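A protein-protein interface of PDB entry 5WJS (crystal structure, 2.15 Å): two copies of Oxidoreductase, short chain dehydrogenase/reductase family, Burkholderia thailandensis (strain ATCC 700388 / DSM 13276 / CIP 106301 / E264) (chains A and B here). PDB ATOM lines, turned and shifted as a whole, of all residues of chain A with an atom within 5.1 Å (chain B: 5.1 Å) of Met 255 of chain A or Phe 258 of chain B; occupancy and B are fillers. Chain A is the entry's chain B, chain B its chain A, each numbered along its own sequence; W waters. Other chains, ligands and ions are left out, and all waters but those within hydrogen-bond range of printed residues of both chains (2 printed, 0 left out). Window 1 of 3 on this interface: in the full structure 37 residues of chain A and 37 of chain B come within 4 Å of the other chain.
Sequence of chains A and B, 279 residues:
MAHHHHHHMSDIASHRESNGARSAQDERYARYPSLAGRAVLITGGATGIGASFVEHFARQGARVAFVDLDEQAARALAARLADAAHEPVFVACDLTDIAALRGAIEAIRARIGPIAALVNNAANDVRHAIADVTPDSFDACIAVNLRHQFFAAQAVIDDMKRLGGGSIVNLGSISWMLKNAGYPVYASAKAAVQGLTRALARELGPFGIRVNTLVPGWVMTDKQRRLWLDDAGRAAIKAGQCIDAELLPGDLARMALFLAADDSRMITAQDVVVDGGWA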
ATOM      1  N   TYR A  32      -6.245  22.229   6.727  1.00  0.00           N
ATOM      2  CA  TYR A  32      -6.265  23.509   7.430  1.00  0.00           C
ATOM      3  C   TYR A  32      -5.442  23.391   8.702  1.00  0.00           C
ATOM      4  O   TYR A  32      -5.937  22.870   9.715  1.00  0.00           O
ATOM      5  CB  TYR A  32      -7.702  23.920   7.764  1.00  0.00           C
ATOM      6  CG  TYR A  32      -8.586  24.108   6.557  1.00  0.00           C
ATOM      7  CD1 TYR A  32      -9.282  23.031   5.999  1.00  0.00           C
ATOM      8  CD2 TYR A  32      -8.728  25.360   5.970  1.00  0.00           C
ATOM      9  CE1 TYR A  32     -10.098  23.205   4.884  1.00  0.00           C
ATOM     10  CE2 TYR A  32      -9.537  25.542   4.864  1.00  0.00           C
ATOM     11  CZ  TYR A  32     -10.217  24.463   4.323  1.00  0.00           C
ATOM     12  OH  TYR A  32     -11.017  24.662   3.214  1.00  0.00           O
ATOM     13  N   LEU A 214     -24.456  29.439   7.362  1.00  0.00           N
ATOM     14  CA  LEU A 214     -24.113  28.528   6.275  1.00  0.00           C
ATOM     15  C   LEU A 214     -25.410  27.976   5.694  1.00  0.00           C
ATOM     16  O   LEU A 214     -26.178  27.332   6.414  1.00  0.00           O
ATOM     17  CB  LEU A 214     -23.205  27.402   6.775  1.00  0.00           C
ATOM     18  CG  LEU A 214     -22.836  26.302   5.777  1.00  0.00           C
ATOM     19  CD1 LEU A 214     -22.041  26.879   4.597  1.00  0.00           C
ATOM     20  CD2 LEU A 214     -22.030  25.259   6.532  1.00  0.00           C
ATOM     21  N   GLY A 250     -20.289  16.565   2.058  1.00  0.00           N
ATOM     22  CA  GLY A 250     -18.924  17.080   2.031  1.00  0.00           C
ATOM     23  C   GLY A 250     -18.793  18.485   1.457  1.00  0.00           C
ATOM     24  O   GLY A 250     -17.916  19.251   1.878  1.00  0.00           O
ATOM     25  N   ASP A 251     -19.636  18.842   0.480  1.00  0.00           N
ATOM     26  CA  ASP A 251     -19.611  20.213  -0.036  1.00  0.00           C
ATOM     27  C   ASP A 251     -19.877  21.221   1.077  1.00  0.00           C
ATOM     28  O   ASP A 251     -19.250  22.287   1.128  1.00  0.00           O
ATOM     29  CB  ASP A 251     -20.642  20.398  -1.147  1.00  0.00           C
ATOM     30  CG  ASP A 251     -20.336  19.574  -2.369  1.00  0.00           C
ATOM     31  OD1 ASP A 251     -21.085  18.618  -2.650  1.00  0.00           O
ATOM     32  OD2 ASP A 251     -19.350  19.890  -3.050  1.00  0.00           O
ATOM     33  N   LEU A 252     -20.800  20.896   1.979  1.00  0.00           N
ATOM     34  CA  LEU A 252     -21.082  21.771   3.106  1.00  0.00           C
ATOM     35  C   LEU A 252     -19.992  21.687   4.162  1.00  0.00           C
ATOM     36  O   LEU A 252     -19.594  22.713   4.727  1.00  0.00           O
ATOM     37  CB  LEU A 252     -22.440  21.424   3.710  1.00  0.00           C
ATOM     38  CG  LEU A 252     -23.662  22.139   3.102  1.00  0.00           C
ATOM     39  CD1 LEU A 252     -23.559  23.633   3.341  1.00  0.00           C
ATOM     40  CD2 LEU A 252     -23.844  21.858   1.602  1.00  0.00           C
ATOM     41  N   ALA A 253     -19.505  20.475   4.443  1.00  0.00           N
ATOM     42  CA  ALA A 253     -18.489  20.303   5.477  1.00  0.00           C
ATOM     43  C   ALA A 253     -17.223  21.094   5.151  1.00  0.00           C
ATOM     44  O   ALA A 253     -16.668  21.777   6.022  1.00  0.00           O
ATOM     45  CB  ALA A 253     -18.168  18.816   5.651  1.00  0.00           C
ATOM     46  N   ARG A 254     -16.762  21.039   3.898  1.00  0.00           N
ATOM     47  CA  ARG A 254     -15.557  21.781   3.542  1.00  0.00           C
ATOM     48  C   ARG A 254     -15.752  23.278   3.755  1.00  0.00           C
ATOM     49  O   ARG A 254     -14.854  23.960   4.268  1.00  0.00           O
ATOM     50  CB  ARG A 254     -15.141  21.473   2.104  1.00  0.00           C
ATOM     51  CG  ARG A 254     -14.587  20.033   1.968  1.00  0.00           C
ATOM     52  CD  ARG A 254     -13.975  19.796   0.584  1.00  0.00           C
ATOM     53  NE  ARG A 254     -14.912  20.163  -0.482  1.00  0.00           N
ATOM     54  CZ  ARG A 254     -15.789  19.319  -1.018  1.00  0.00           C
ATOM     55  NH1 ARG A 254     -15.843  18.066  -0.587  1.00  0.00           N
ATOM     56  NH2 ARG A 254     -16.609  19.723  -1.989  1.00  0.00           N
ATOM     57  N   MET A 255     -16.931  23.806   3.406  1.00  0.00           N
ATOM     58  CA  MET A 255     -17.165  25.226   3.639  1.00  0.00           C
ATOM     59  C   MET A 255     -17.112  25.552   5.127  1.00  0.00           C
ATOM     60  O   MET A 255     -16.572  26.592   5.523  1.00  0.00           O
ATOM     61  CB  MET A 255     -18.505  25.658   3.047  1.00  0.00           C
ATOM     62  CG  MET A 255     -18.690  27.171   3.036  1.00  0.00           C
ATOM     63  SD  MET A 255     -17.611  27.954   1.826  1.00  0.00           S
ATOM     64  CE  MET A 255     -16.421  28.807   2.903  1.00  0.00           C
ATOM     65  N   ALA A 256     -17.670  24.674   5.968  1.00  0.00           N
ATOM     66  CA  ALA A 256     -17.598  24.882   7.412  1.00  0.00           C
ATOM     67  C   ALA A 256     -16.153  24.870   7.913  1.00  0.00           C
ATOM     68  O   ALA A 256     -15.806  25.627   8.827  1.00  0.00           O
ATOM     69  CB  ALA A 256     -18.414  23.810   8.139  1.00  0.00           C
ATOM     70  N   LEU A 257     -15.313  23.990   7.357  1.00  0.00           N
ATOM     71  CA  LEU A 257     -13.906  23.952   7.751  1.00  0.00           C
ATOM     72  C   LEU A 257     -13.247  25.303   7.510  1.00  0.00           C
ATOM     73  O   LEU A 257     -12.568  25.841   8.393  1.00  0.00           O
ATOM     74  CB  LEU A 257     -13.155  22.857   6.979  1.00  0.00           C
ATOM     75  CG  LEU A 257     -13.457  21.364   7.180  1.00  0.00           C
ATOM     76  CD1 LEU A 257     -12.533  20.531   6.293  1.00  0.00           C
ATOM     77  CD2 LEU A 257     -13.328  20.935   8.628  1.00  0.00           C
ATOM     78  N   PHE A 258     -13.432  25.855   6.303  1.00  0.00           N
ATOM     79  CA  PHE A 258     -12.872  27.156   5.958  1.00  0.00           C
ATOM     80  C   PHE A 258     -13.403  28.245   6.888  1.00  0.00           C
ATOM     81  O   PHE A 258     -12.647  29.119   7.323  1.00  0.00           O
ATOM     82  CB  PHE A 258     -13.193  27.468   4.492  1.00  0.00           C
ATOM     83  CG  PHE A 258     -12.601  28.759   3.980  1.00  0.00           C
ATOM     84  CD1 PHE A 258     -13.281  29.967   4.148  1.00  0.00           C
ATOM     85  CD2 PHE A 258     -11.379  28.760   3.295  1.00  0.00           C
ATOM     86  CE1 PHE A 258     -12.738  31.159   3.669  1.00  0.00           C
ATOM     87  CE2 PHE A 258     -10.837  29.937   2.804  1.00  0.00           C
ATOM     88  CZ  PHE A 258     -11.525  31.143   2.987  1.00  0.00           C
ATOM     89  N   LEU A 259     -14.700  28.190   7.222  1.00  0.00           N
ATOM     90  CA  LEU A 259     -15.306  29.216   8.077  1.00  0.00           C
ATOM     91  C   LEU A 259     -14.824  29.128   9.526  1.00  0.00           C
ATOM     92  O   LEU A 259     -14.784  30.147  10.230  1.00  0.00           O
ATOM     93  CB  LEU A 259     -16.826  29.104   8.013  1.00  0.00           C
ATOM     94  CG  LEU A 259     -17.457  29.516   6.673  1.00  0.00           C
ATOM     95  CD1 LEU A 259     -18.959  29.219   6.655  1.00  0.00           C
ATOM     96  CD2 LEU A 259     -17.186  31.003   6.388  1.00  0.00           C
ATOM     97  N   VAL A 272     -23.590  32.299   3.706  1.00  0.00           N
ATOM     98  CA  VAL A 272     -22.667  31.572   2.847  1.00  0.00           C
ATOM     99  C   VAL A 272     -23.435  30.402   2.235  1.00  0.00           C
ATOM    100  O   VAL A 272     -23.743  29.422   2.918  1.00  0.00           O
ATOM    101  CB  VAL A 272     -21.435  31.105   3.634  1.00  0.00           C
ATOM    102  CG1 VAL A 272     -20.417  30.454   2.712  1.00  0.00           C
ATOM    103  CG2 VAL A 272     -20.802  32.307   4.372  1.00  0.00           C
ATOM    104  N   VAL A 274     -24.143  27.282  -0.218  1.00  0.00           N
ATOM    105  CA  VAL A 274     -23.513  26.163  -0.930  1.00  0.00           C
ATOM    106  C   VAL A 274     -24.660  25.327  -1.483  1.00  0.00           C
ATOM    107  O   VAL A 274     -25.195  24.455  -0.793  1.00  0.00           O
ATOM    108  CB  VAL A 274     -22.605  25.327  -0.019  1.00  0.00           C
ATOM    109  CG1 VAL A 274     -21.883  24.215  -0.801  1.00  0.00           C
ATOM    110  CG2 VAL A 274     -21.617  26.220   0.737  1.00  0.00           C
ATOM    111  N   TYR B  32      -3.997  23.961  -0.783  1.00  0.00           N
ATOM    112  CA  TYR B  32      -5.031  23.381  -1.645  1.00  0.00           C
ATOM    113  C   TYR B  32      -4.375  22.482  -2.680  1.00  0.00           C
ATOM    114  O   TYR B  32      -3.864  22.984  -3.692  1.00  0.00           O
ATOM    115  CB  TYR B  32      -5.838  24.483  -2.340  1.00  0.00           C
ATOM    116  CG  TYR B  32      -6.574  25.404  -1.395  1.00  0.00           C
ATOM    117  CD1 TYR B  32      -5.933  26.492  -0.810  1.00  0.00           C
ATOM    118  CD2 TYR B  32      -7.909  25.177  -1.074  1.00  0.00           C
ATOM    119  CE1 TYR B  32      -6.607  27.337   0.060  1.00  0.00           C
ATOM    120  CE2 TYR B  32      -8.586  26.007  -0.202  1.00  0.00           C
ATOM    121  CZ  TYR B  32      -7.932  27.089   0.360  1.00  0.00           C
ATOM    122  OH  TYR B  32      -8.604  27.918   1.225  1.00  0.00           O
ATOM    123  N   ARG B 254      -7.167  34.395  -0.007  1.00  0.00           N
ATOM    124  CA  ARG B 254      -7.478  33.058   0.492  1.00  0.00           C
ATOM    125  C   ARG B 254      -8.869  32.615   0.061  1.00  0.00           C
ATOM    126  O   ARG B 254      -9.073  31.440  -0.259  1.00  0.00           O
ATOM    127  CB  ARG B 254      -7.326  33.005   2.013  1.00  0.00           C
ATOM    128  CG  ARG B 254      -5.842  33.106   2.464  1.00  0.00           C
ATOM    129  CD  ARG B 254      -5.670  32.839   3.945  1.00  0.00           C
ATOM    130  NE  ARG B 254      -6.526  33.692   4.771  1.00  0.00           N
ATOM    131  CZ  ARG B 254      -6.182  34.896   5.227  1.00  0.00           C
ATOM    132  NH1 ARG B 254      -4.987  35.406   4.938  1.00  0.00           N
ATOM    133  NH2 ARG B 254      -7.039  35.594   5.975  1.00  0.00           N
ATOM    134  N   MET B 255      -9.838  33.539   0.026  1.00  0.00           N
ATOM    135  CA  MET B 255     -11.168  33.180  -0.455  1.00  0.00           C
ATOM    136  C   MET B 255     -11.133  32.805  -1.929  1.00  0.00           C
ATOM    137  O   MET B 255     -11.822  31.866  -2.356  1.00  0.00           O
ATOM    138  CB  MET B 255     -12.148  34.330  -0.221  1.00  0.00           C
ATOM    139  CG  MET B 255     -13.642  33.950  -0.445  1.00  0.00           C
ATOM    140  SD  MET B 255     -14.230  32.837   0.865  1.00  0.00           S
ATOM    141  CE  MET B 255     -14.415  31.298  -0.042  1.00  0.00           C
ATOM    142  N   ALA B 256     -10.334  33.528  -2.723  1.00  0.00           N
ATOM    143  CA  ALA B 256     -10.205  33.208  -4.139  1.00  0.00           C
ATOM    144  C   ALA B 256      -9.575  31.833  -4.336  1.00  0.00           C
ATOM    145  O   ALA B 256      -9.961  31.095  -5.249  1.00  0.00           O
ATOM    146  CB  ALA B 256      -9.368  34.279  -4.849  1.00  0.00           C
ATOM    147  N   LEU B 257      -8.579  31.490  -3.508  1.00  0.00           N
ATOM    148  CA  LEU B 257      -7.967  30.162  -3.570  1.00  0.00           C
ATOM    149  C   LEU B 257      -9.018  29.073  -3.405  1.00  0.00           C
ATOM    150  O   LEU B 257      -9.088  28.129  -4.199  1.00  0.00           O
ATOM    151  CB  LEU B 257      -6.890  30.023  -2.487  1.00  0.00           C
ATOM    152  CG  LEU B 257      -5.573  30.796  -2.587  1.00  0.00           C
ATOM    153  CD1 LEU B 257      -4.691  30.395  -1.428  1.00  0.00           C
ATOM    154  CD2 LEU B 257      -4.832  30.570  -3.917  1.00  0.00           C
ATOM    155  N   PHE B 258      -9.848  29.199  -2.371  1.00  0.00           N
ATOM    156  CA  PHE B 258     -10.913  28.233  -2.119  1.00  0.00           C
ATOM    157  C   PHE B 258     -11.889  28.167  -3.288  1.00  0.00           C
ATOM    158  O   PHE B 258     -12.280  27.073  -3.721  1.00  0.00           O
ATOM    159  CB  PHE B 258     -11.619  28.614  -0.810  1.00  0.00           C
ATOM    160  CG  PHE B 258     -12.679  27.626  -0.350  1.00  0.00           C
ATOM    161  CD1 PHE B 258     -13.990  27.727  -0.815  1.00  0.00           C
ATOM    162  CD2 PHE B 258     -12.375  26.646   0.583  1.00  0.00           C
ATOM    163  CE1 PHE B 258     -14.970  26.834  -0.375  1.00  0.00           C
ATOM    164  CE2 PHE B 258     -13.341  25.746   1.032  1.00  0.00           C
ATOM    165  CZ  PHE B 258     -14.644  25.846   0.548  1.00  0.00           C
ATOM    166  N   LEU B 259     -12.275  29.326  -3.832  1.00  0.00           N
ATOM    167  CA  LEU B 259     -13.246  29.346  -4.919  1.00  0.00           C
ATOM    168  C   LEU B 259     -12.697  28.717  -6.191  1.00  0.00           C
ATOM    169  O   LEU B 259     -13.472  28.256  -7.038  1.00  0.00           O
ATOM    170  CB  LEU B 259     -13.689  30.778  -5.215  1.00  0.00           C
ATOM    171  CG  LEU B 259     -14.612  31.383  -4.157  1.00  0.00           C
ATOM    172  CD1 LEU B 259     -14.987  32.816  -4.550  1.00  0.00           C
ATOM    173  CD2 LEU B 259     -15.835  30.514  -3.993  1.00  0.00           C
ATOM    174  N   ALA B 260     -11.381  28.739  -6.369  1.00  0.00           N
ATOM    175  CA  ALA B 260     -10.782  28.190  -7.574  1.00  0.00           C
ATOM    176  C   ALA B 260     -10.376  26.741  -7.395  1.00  0.00           C
ATOM    177  O   ALA B 260     -10.235  26.021  -8.393  1.00  0.00           O
ATOM    178  CB  ALA B 260      -9.562  29.020  -7.991  1.00  0.00           C
ATOM    179  N   ALA B 261     -10.189  26.307  -6.149  1.00  0.00           N
ATOM    180  CA  ALA B 261      -9.803  24.938  -5.854  1.00  0.00           C
ATOM    181  C   ALA B 261     -11.001  24.000  -5.997  1.00  0.00           C
ATOM    182  O   ALA B 261     -12.155  24.429  -5.991  1.00  0.00           O
ATOM    183  CB  ALA B 261      -9.233  24.851  -4.444  1.00  0.00           C
ATOM    184  N   ASP B 263     -12.251  22.311  -3.827  1.00  0.00           N
ATOM    185  CA  ASP B 263     -13.045  22.320  -2.597  1.00  0.00           C
ATOM    186  C   ASP B 263     -14.388  23.037  -2.755  1.00  0.00           C
ATOM    187  O   ASP B 263     -15.299  22.810  -1.950  1.00  0.00           O
ATOM    188  CB  ASP B 263     -12.243  22.980  -1.470  1.00  0.00           C
ATOM    189  CG  ASP B 263     -10.848  22.389  -1.318  1.00  0.00           C
ATOM    190  OD1 ASP B 263     -10.072  22.398  -2.306  1.00  0.00           O
ATOM    191  OD2 ASP B 263     -10.535  21.916  -0.206  1.00  0.00           O
ATOM    192  N   SER B 264     -14.536  23.887  -3.770  1.00  0.00           N
ATOM    193  CA  SER B 264     -15.727  24.709  -3.947  1.00  0.00           C
ATOM    194  C   SER B 264     -16.552  24.300  -5.177  1.00  0.00           C
ATOM    195  O   SER B 264     -17.268  25.125  -5.754  1.00  0.00           O
ATOM    196  CB  SER B 264     -15.314  26.174  -4.030  1.00  0.00           C
ATOM    197  OG  SER B 264     -14.516  26.400  -5.183  1.00  0.00           O
ATOM    198  N   ILE B 267     -20.191  25.524  -5.343  1.00  0.00           N
ATOM    199  CA  ILE B 267     -20.482  26.927  -5.080  1.00  0.00           C
ATOM    200  C   ILE B 267     -20.442  27.679  -6.406  1.00  0.00           C
ATOM    201  O   ILE B 267     -19.390  27.763  -7.051  1.00  0.00           O
ATOM    202  CB  ILE B 267     -19.494  27.530  -4.070  1.00  0.00           C
ATOM    203  CG1 ILE B 267     -19.596  26.796  -2.737  1.00  0.00           C
ATOM    204  CG2 ILE B 267     -19.775  29.035  -3.894  1.00  0.00           C
ATOM    205  CD1 ILE B 267     -18.534  27.186  -1.744  1.00  0.00           C
HETATM  206  O   HOH W   1     -17.803  23.630  -0.893  1.00  0.00           O
HETATM  207  O   HOH W   2     -11.853  22.432   2.095  1.00  0.00           O
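The backbone carbonyl oxygen of Asp 263 of chain B is in hydrogen-bond range of the guanidinium group of Arg 254 of chain A, 3.1 Å away.
OG of Ser 264 of chain B lies within hydrogen-bond range of O of Phe 258 of chain B. The guanidinium group (NH1) of Arg 254 of chain A lies close to the backbone carbonyl oxygen (O) of Gly 250 of chain A (3.4 Å). OD2 of Asp 251 of chain A is in salt-bridge range of NH2 of Arg 254 of chain A (2.9 Å).
Among the printed residues, pairs that only touch across the chains: Tyr 32 of chain A with Phe 258 of chain B (3.4 Å), Phe 258 of chain A with Tyr 32 of chain B (3.4 Å), Phe 258 of chain A with Phe 258 of chain B (3.6 Å), Phe 258 of chain A with Met 255 of chain B (3.6 Å), Met 255 of chain A with Phe 258 of chain B (3.6 Å), Met 255 of chain A with Ile 267 of chain B (3.8 Å), Phe 258 of chain A with Arg 254 of chain B (3.8 Å), Val 274 of chain A with Ile 267 of chain B (3.95 Å) and Arg 254 of chain A with Phe 258 of chain B (3.99 Å).
Ala 253 of chain A touches none of the printed residues of chain B. Met 255 of chain A touches two residues of chain B. Leu 257 of chain A touches none of the printed residues of chain B. Of the printed residues of chain B, Val 274 of chain A touches Ile 267. Of the printed residues of chain A, Phe 258 of chain B touches Tyr 32 (3.4 Å), Arg 254 (3.99 Å), Met 255 (3.6 Å) and Phe 258 (3.6 Å). Of the printed residues of chain A, Asp 263 of chain B touches Arg 254 (3.1 Å). The nearest residue of chain B that does not touch Met 255 of chain A is Met 255 of chain B (4.3 Å).
Of the 12 printed residues of chain B, 6 touch a printed residue of chain A. Along chain B the printed residues that touch a printed residue of chain A span positions 32 to 267.
Tyr 32 of chain A touches Phe 258 of chain B, and with the chains exchanged Phe 258 of chain A touches Tyr 32 of chain B. Arg 254 of chain A touches Phe 258 of chain B, and with the chains exchanged Phe 258 of chain A touches Arg 254 of chain B. Met 255 of chain A touches Phe 258 of chain B, and with the chains exchanged Phe 258 of chain A touches Met 255 of chain B. Phe 258 of chain B touches its own counterpart, Phe 258 of chain A. 7 positions are printed for both chains.
Water W2 bridges OH of Tyr 32 of chain A and OD2 of Asp 263 of chain B. Water W1 lies within hydrogen-bond range of O of Asp 251 of chain A and O of Asp 263 of chain B.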
